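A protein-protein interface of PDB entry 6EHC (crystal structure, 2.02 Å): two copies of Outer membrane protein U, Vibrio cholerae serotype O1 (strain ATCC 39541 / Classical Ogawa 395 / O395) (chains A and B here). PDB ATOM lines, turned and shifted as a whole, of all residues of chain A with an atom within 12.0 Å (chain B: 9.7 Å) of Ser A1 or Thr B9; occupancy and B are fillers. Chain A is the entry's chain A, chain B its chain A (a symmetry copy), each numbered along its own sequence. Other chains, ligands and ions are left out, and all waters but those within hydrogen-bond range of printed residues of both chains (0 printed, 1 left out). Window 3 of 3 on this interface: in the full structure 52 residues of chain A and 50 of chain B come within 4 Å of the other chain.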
ATOM      1  N   SER A   1       4.479 -26.762  22.776  1.00  0.00           N
ATOM      2  CA  SER A   1       4.325 -28.224  22.435  1.00  0.00           C
ATOM      3  C   SER A   1       4.065 -28.430  20.922  1.00  0.00           C
ATOM      4  O   SER A   1       3.400 -29.349  20.509  1.00  0.00           O
ATOM      5  CB  SER A   1       3.208 -28.859  23.293  1.00  0.00           C
ATOM      6  OG  SER A   1       3.719 -29.851  24.172  1.00  0.00           O
ATOM      7  N   THR A   2       4.663 -27.598  20.098  1.00  0.00           N
ATOM      8  CA  THR A   2       4.178 -27.419  18.759  1.00  0.00           C
ATOM      9  C   THR A   2       5.053 -28.257  17.735  1.00  0.00           C
ATOM     10  O   THR A   2       6.266 -28.209  17.755  1.00  0.00           O
ATOM     11  CB  THR A   2       4.052 -25.896  18.604  1.00  0.00           C
ATOM     12  OG1 THR A   2       2.997 -25.552  17.696  1.00  0.00           O
ATOM     13  CG2 THR A   2       5.359 -25.276  18.215  1.00  0.00           C
ATOM     14  N   VAL A   3       4.420 -29.069  16.886  1.00  0.00           N
ATOM     15  CA  VAL A   3       5.115 -30.013  15.990  1.00  0.00           C
ATOM     16  C   VAL A   3       5.058 -29.538  14.519  1.00  0.00           C
ATOM     17  O   VAL A   3       3.948 -29.385  13.996  1.00  0.00           O
ATOM     18  CB  VAL A   3       4.505 -31.440  16.100  1.00  0.00           C
ATOM     19  CG1 VAL A   3       5.231 -32.454  15.218  1.00  0.00           C
ATOM     20  CG2 VAL A   3       4.490 -31.941  17.560  1.00  0.00           C
ATOM     21  N   TYR A   4       6.219 -29.368  13.851  1.00  0.00           N
ATOM     22  CA  TYR A   4       6.267 -28.881  12.448  1.00  0.00           C
ATOM     23  C   TYR A   4       6.896 -29.846  11.458  1.00  0.00           C
ATOM     24  O   TYR A   4       7.811 -30.608  11.796  1.00  0.00           O
ATOM     25  CB  TYR A   4       7.040 -27.581  12.339  1.00  0.00           C
ATOM     26  CG  TYR A   4       6.522 -26.477  13.200  1.00  0.00           C
ATOM     27  CD1 TYR A   4       5.499 -25.637  12.764  1.00  0.00           C
ATOM     28  CD2 TYR A   4       7.067 -26.253  14.459  1.00  0.00           C
ATOM     29  CE1 TYR A   4       5.011 -24.606  13.565  1.00  0.00           C
ATOM     30  CE2 TYR A   4       6.595 -25.230  15.266  1.00  0.00           C
ATOM     31  CZ  TYR A   4       5.566 -24.408  14.825  1.00  0.00           C
ATOM     32  OH  TYR A   4       5.099 -23.387  15.623  1.00  0.00           O
ATOM     33  N   SER A   5       6.444 -29.761  10.203  1.00  0.00           N
ATOM     34  CA  SER A   5       7.111 -30.456   9.102  1.00  0.00           C
ATOM     35  C   SER A   5       8.329 -29.632   8.651  1.00  0.00           C
ATOM     36  O   SER A   5       8.226 -28.413   8.475  1.00  0.00           O
ATOM     37  CB  SER A   5       6.166 -30.685   7.923  1.00  0.00           C
ATOM     38  OG  SER A   5       5.568 -29.503   7.412  1.00  0.00           O
ATOM     39  N   THR B   2      -4.746 -32.124  15.991  1.00  0.00           N
ATOM     40  CA  THR B   2      -3.645 -31.298  16.399  1.00  0.00           C
ATOM     41  C   THR B   2      -2.504 -32.179  17.062  1.00  0.00           C
ATOM     42  O   THR B   2      -2.759 -32.999  17.920  1.00  0.00           O
ATOM     43  CB  THR B   2      -4.302 -30.159  17.194  1.00  0.00           C
ATOM     44  OG1 THR B   2      -3.548 -28.946  17.085  1.00  0.00           O
ATOM     45  CG2 THR B   2      -4.538 -30.553  18.620  1.00  0.00           C
ATOM     46  N   VAL B   3      -1.259 -32.040  16.604  1.00  0.00           N
ATOM     47  CA  VAL B   3      -0.136 -32.902  17.023  1.00  0.00           C
ATOM     48  C   VAL B   3       0.841 -32.142  17.950  1.00  0.00           C
ATOM     49  O   VAL B   3       1.387 -31.122  17.513  1.00  0.00           O
ATOM     50  CB  VAL B   3       0.637 -33.452  15.789  1.00  0.00           C
ATOM     51  CG1 VAL B   3       1.779 -34.385  16.186  1.00  0.00           C
ATOM     52  CG2 VAL B   3      -0.305 -34.175  14.804  1.00  0.00           C
ATOM     53  N   TYR B   4       1.101 -32.655  19.171  1.00  0.00           N
ATOM     54  CA  TYR B   4       1.998 -31.979  20.145  1.00  0.00           C
ATOM     55  C   TYR B   4       3.221 -32.783  20.552  1.00  0.00           C
ATOM     56  O   TYR B   4       3.184 -34.018  20.620  1.00  0.00           O
ATOM     57  CB  TYR B   4       1.263 -31.628  21.424  1.00  0.00           C
ATOM     58  CG  TYR B   4       0.052 -30.774  21.230  1.00  0.00           C
ATOM     59  CD1 TYR B   4       0.148 -29.384  21.176  1.00  0.00           C
ATOM     60  CD2 TYR B   4      -1.205 -31.354  21.115  1.00  0.00           C
ATOM     61  CE1 TYR B   4      -0.977 -28.583  20.994  1.00  0.00           C
ATOM     62  CE2 TYR B   4      -2.334 -30.571  20.937  1.00  0.00           C
ATOM     63  CZ  TYR B   4      -2.225 -29.187  20.872  1.00  0.00           C
ATOM     64  OH  TYR B   4      -3.346 -28.407  20.701  1.00  0.00           O
ATOM     65  N   SER B   5       4.295 -32.065  20.892  1.00  0.00           N
ATOM     66  CA  SER B   5       5.460 -32.686  21.524  1.00  0.00           C
ATOM     67  C   SER B   5       5.183 -32.866  23.026  1.00  0.00           C
ATOM     68  O   SER B   5       4.700 -31.939  23.685  1.00  0.00           O
ATOM     69  CB  SER B   5       6.724 -31.853  21.318  1.00  0.00           C
ATOM     70  OG  SER B   5       6.627 -30.513  21.778  1.00  0.00           O
ATOM     71  N   ALA B   6       5.539 -34.032  23.563  1.00  0.00           N
ATOM     72  CA  ALA B   6       5.301 -34.359  24.981  1.00  0.00           C
ATOM     73  C   ALA B   6       5.969 -33.387  25.951  1.00  0.00           C
ATOM     74  O   ALA B   6       5.331 -32.883  26.839  1.00  0.00           O
ATOM     75  CB  ALA B   6       5.724 -35.822  25.261  1.00  0.00           C
ATOM     76  N   LYS B   7       7.247 -33.092  25.733  1.00  0.00           N
ATOM     77  CA  LYS B   7       8.065 -32.325  26.658  1.00  0.00           C
ATOM     78  C   LYS B   7       8.779 -31.119  26.064  1.00  0.00           C
ATOM     79  O   LYS B   7       9.103 -30.208  26.826  1.00  0.00           O
ATOM     80  CB  LYS B   7       9.124 -33.246  27.253  1.00  0.00           C
ATOM     81  CG  LYS B   7       8.629 -34.194  28.321  1.00  0.00           C
ATOM     82  CD  LYS B   7       9.384 -35.502  28.253  1.00  0.00           C
ATOM     83  CE  LYS B   7      10.077 -35.871  29.548  1.00  0.00           C
ATOM     84  NZ  LYS B   7       9.095 -36.052  30.650  1.00  0.00           N
ATOM     85  N   GLY B   8       9.061 -31.108  24.739  1.00  0.00           N
ATOM     86  CA  GLY B   8       9.824 -30.016  24.095  1.00  0.00           C
ATOM     87  C   GLY B   8       8.979 -28.773  23.841  1.00  0.00           C
ATOM     88  O   GLY B   8       7.755 -28.836  23.905  1.00  0.00           O
ATOM     89  N   THR B   9       9.614 -27.632  23.551  1.00  0.00           N
ATOM     90  CA  THR B   9       8.852 -26.440  23.089  1.00  0.00           C
ATOM     91  C   THR B   9       8.391 -26.730  21.626  1.00  0.00           C
ATOM     92  O   THR B   9       7.252 -26.334  21.194  1.00  0.00           O
ATOM     93  CB  THR B   9       9.635 -25.077  23.259  1.00  0.00           C
ATOM     94  OG1 THR B   9      10.813 -25.010  22.409  1.00  0.00           O
ATOM     95  CG2 THR B   9      10.069 -24.870  24.740  1.00  0.00           C
ATOM     96  N   SER B  10       9.253 -27.438  20.879  1.00  0.00           N
ATOM     97  CA  SER B  10       8.900 -27.868  19.510  1.00  0.00           C
ATOM     98  C   SER B  10       9.714 -29.045  18.988  1.00  0.00           C
ATOM     99  O   SER B  10      10.845 -29.339  19.450  1.00  0.00           O
ATOM    100  CB  SER B  10       9.106 -26.723  18.519  1.00  0.00           C
ATOM    101  OG  SER B  10      10.506 -26.440  18.395  1.00  0.00           O
ATOM    102  N   LEU B  11       9.141 -29.669  17.970  1.00  0.00           N
ATOM    103  CA  LEU B  11       9.700 -30.860  17.360  1.00  0.00           C
ATOM    104  C   LEU B  11       9.549 -30.664  15.859  1.00  0.00           C
ATOM    105  O   LEU B  11       8.457 -30.250  15.412  1.00  0.00           O
ATOM    106  CB  LEU B  11       8.923 -32.064  17.828  1.00  0.00           C
ATOM    107  CG  LEU B  11       9.249 -33.400  17.181  1.00  0.00           C
ATOM    108  CD1 LEU B  11      10.680 -33.794  17.484  1.00  0.00           C
ATOM    109  CD2 LEU B  11       8.322 -34.433  17.705  1.00  0.00           C
ATOM    110  N   GLU B  12      10.633 -30.893  15.115  1.00  0.00           N
ATOM    111  CA  GLU B  12      10.593 -30.836  13.640  1.00  0.00           C
ATOM    112  C   GLU B  12      10.684 -32.281  13.094  1.00  0.00           C
ATOM    113  O   GLU B  12      11.569 -33.044  13.485  1.00  0.00           O
ATOM    114  CB  GLU B  12      11.670 -29.905  13.108  1.00  0.00           C
ATOM    115  CG  GLU B  12      11.815 -29.798  11.596  1.00  0.00           C
ATOM    116  CD  GLU B  12      12.790 -28.682  11.217  1.00  0.00           C
ATOM    117  OE1 GLU B  12      13.855 -28.967  10.677  1.00  0.00           O
ATOM    118  OE2 GLU B  12      12.511 -27.519  11.543  1.00  0.00           O
ATOM    119  N   LEU B  39      13.941 -33.826  15.090  1.00  0.00           N
ATOM    120  CA  LEU B  39      14.932 -32.854  15.572  1.00  0.00           C
ATOM    121  C   LEU B  39      14.303 -32.047  16.665  1.00  0.00           C
ATOM    122  O   LEU B  39      13.307 -31.352  16.424  1.00  0.00           O
ATOM    123  CB  LEU B  39      15.355 -31.870  14.441  1.00  0.00           C
ATOM    124  CG  LEU B  39      16.346 -30.746  14.778  1.00  0.00           C
ATOM    125  CD1 LEU B  39      17.641 -31.354  15.277  1.00  0.00           C
ATOM    126  CD2 LEU B  39      16.651 -29.863  13.558  1.00  0.00           C
ATOM    127  N   GLY B  40      14.908 -32.106  17.855  1.00  0.00           N
ATOM    128  CA  GLY B  40      14.443 -31.326  18.994  1.00  0.00           C
ATOM    129  C   GLY B  40      15.540 -30.391  19.447  1.00  0.00           C
ATOM    130  O   GLY B  40      16.728 -30.775  19.464  1.00  0.00           O
ATOM    131  N   LYS B  41      15.141 -29.197  19.855  1.00  0.00           N
ATOM    132  CA  LYS B  41      16.073 -28.181  20.344  1.00  0.00           C
ATOM    133  C   LYS B  41      15.511 -27.451  21.580  1.00  0.00           C
ATOM    134  O   LYS B  41      14.355 -27.036  21.603  1.00  0.00           O
ATOM    135  CB  LYS B  41      16.372 -27.194  19.238  1.00  0.00           C
ATOM    136  CG  LYS B  41      17.524 -26.240  19.487  1.00  0.00           C
ATOM    137  CD  LYS B  41      17.855 -25.388  18.233  1.00  0.00           C
ATOM    138  CE  LYS B  41      18.542 -24.051  18.567  1.00  0.00           C
ATOM    139  NZ  LYS B  41      19.147 -23.423  17.350  1.00  0.00           N
ATOM    140  N   ALA B  42      16.348 -27.289  22.588  1.00  0.00           N
ATOM    141  CA  ALA B  42      15.967 -26.667  23.857  1.00  0.00           C
ATOM    142  C   ALA B  42      16.842 -25.462  24.050  1.00  0.00           C
ATOM    143  O   ALA B  42      18.056 -25.609  24.372  1.00  0.00           O
ATOM    144  CB  ALA B  42      16.215 -27.643  25.001  1.00  0.00           C
ATOM    145  N   GLU B  43      16.259 -24.285  23.856  1.00  0.00           N
ATOM    146  CA  GLU B  43      16.937 -23.035  24.197  1.00  0.00           C
ATOM    147  C   GLU B  43      17.149 -22.911  25.699  1.00  0.00           C
ATOM    148  O   GLU B  43      16.197 -23.088  26.470  1.00  0.00           O
ATOM    149  CB  GLU B  43      16.179 -21.844  23.655  1.00  0.00           C
ATOM    150  CG  GLU B  43      16.338 -21.777  22.155  1.00  0.00           C
ATOM    151  CD  GLU B  43      15.403 -20.772  21.537  1.00  0.00           C
ATOM    152  OE1 GLU B  43      15.236 -19.675  22.147  1.00  0.00           O
ATOM    153  OE2 GLU B  43      14.848 -21.101  20.460  1.00  0.00           O
ATOM    154  N   ILE B  44      18.408 -22.701  26.089  1.00  0.00           N
ATOM    155  CA  ILE B  44      18.810 -22.558  27.509  1.00  0.00           C
ATOM    156  C   ILE B  44      18.936 -21.071  27.886  1.00  0.00           C
ATOM    157  O   ILE B  44      18.298 -20.614  28.817  1.00  0.00           O
ATOM    158  CB  ILE B  44      20.115 -23.344  27.816  1.00  0.00           C
ATOM    159  CG1 ILE B  44      19.923 -24.825  27.463  1.00  0.00           C
ATOM    160  CG2 ILE B  44      20.510 -23.173  29.298  1.00  0.00           C
ATOM    161  CD1 ILE B  44      21.182 -25.634  27.339  1.00  0.00           C
ATOM    162  N   GLY B  50      20.452 -26.996  23.882  1.00  0.00           N
ATOM    163  CA  GLY B  50      20.614 -28.437  23.781  1.00  0.00           C
ATOM    164  C   GLY B  50      19.891 -28.938  22.521  1.00  0.00           C
ATOM    165  O   GLY B  50      18.941 -28.290  22.066  1.00  0.00           O
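Of chain B, only Tyr B4 (3.0 Å), Ser B5 (2.4 Å), Gly B8 (3.8 Å) and Thr B9 (3.2 Å) come within 4 Å of Ser A1.
Of chain A, only Ser A1 and Thr A2 come within 4 Å of Thr B9.
Thr A2 touches just these residues of chain B: Ser B5 (3.9 Å), Thr B9 (3.1 Å), Ser B10 (3.2 Å) and Leu B11 (3.2 Å).
Ala B6 touches none of the printed residues of chain A.
Of chain A, only Ser A1 (3.8 Å) comes within 4 Å of Gly B8.
Of chain A, only Thr A2 (3.2 Å) comes within 4 Å of Ser B10.
No residue of chain A comes within 4 Å of Ala B42.
No residue of chain A comes within 4 Å of Glu B43.
Printed residues of chain A within 4 Å of Leu B11: Thr A2, Val A3 and Tyr A4.
Printed residues of chain B within 4 Å of Tyr A4: Leu B11 and Glu B12.
Of the printed residues of chain B, Val A3 touches Val B3, Tyr B4, Ser B5 and Leu B11.
The nearest residue of chain B that does not touch Ser A1 is Val B3 (4.02 Å).
The nearest residue of chain A that does not touch Thr B9 is Val A3 (5.8 Å).
O of Ser A1 is in hydrogen-bond range of N of Ser B5, 2.9 Å away.
The backbone NH (N) of Ser A1 sits at hydrogen-bond distance from the backbone carbonyl oxygen (O) of Thr B9 (3.2 Å).
The backbone NH of Thr A2 sits at hydrogen-bond distance from the backbone carbonyl oxygen of Thr B9 (3.1 Å).
O of Thr A2 is in hydrogen-bond range of N of Leu B11, at 3.2 Å.
The backbone carbonyl oxygen (O) of Leu B11 is in hydrogen-bond range of the backbone NH (N) of Tyr A4 (2.9 Å).
Thr A2 touches Ser B5, but with the chains exchanged Ser A5 does not touch Thr B2 (11.5 Å).
Val A3 touches its own counterpart, Val B3.
Val A3 touches Tyr B4, but with the chains exchanged Tyr A4 does not touch Val B3 (6.3 Å).
Val A3 touches Ser B5, but with the chains exchanged Ser A5 does not touch Val B3 (8.9 Å).
Of the 14 pairs that touch across the chains among the printed residues, 1 has its exchanged pair printed and touching as well.
Hydrophobic or aromatic side chains of chain A that line the printed part of chain B: Val A3.
Along chain A the printed residues that touch a printed residue of chain B span positions 1 to 4.
Hydrophobic or aromatic side chains of chain B within 4 Å of the printed part of chain A: Val B3 and Tyr B4.
Along chain B the printed residues that touch a printed residue of chain A span positions 3 to 12.
Among the printed residues, no Asp or Glu carboxylate lies within 4 Å of a Lys or Arg side-chain nitrogen of the other chain.
The backbone carbonyl oxygen (O) of Gly B8 lies within hydrogen-bond range of the side-chain hydroxyl (OG) of Ser B5 (2.9 Å).
The backbone NH (N) of Leu B39 is in hydrogen-bond range of the backbone carbonyl oxygen (O) of Glu B12.
Ser A1 touches Tyr B4 (O to CA, 3.0 Å).
O of Gly B8 touches CA of Ser A1 (3.8 Å).
Ser B5 touches Thr A2 (OG to N, 3.9 Å).
O of Thr A2 touches CA of Ser B10, at 3.2 Å.
CG2 of Val A3 touches O of Val B3 (3.2 Å).
Tyr B4 touches Val A3 (C to CG2, 3.4 Å).
Ser B5 touches Val A3 (N to CG2, 3.3 Å).
Leu B11 touches Val A3.
CA of Glu B12 touches O of Tyr A4, at 3.3 Å.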
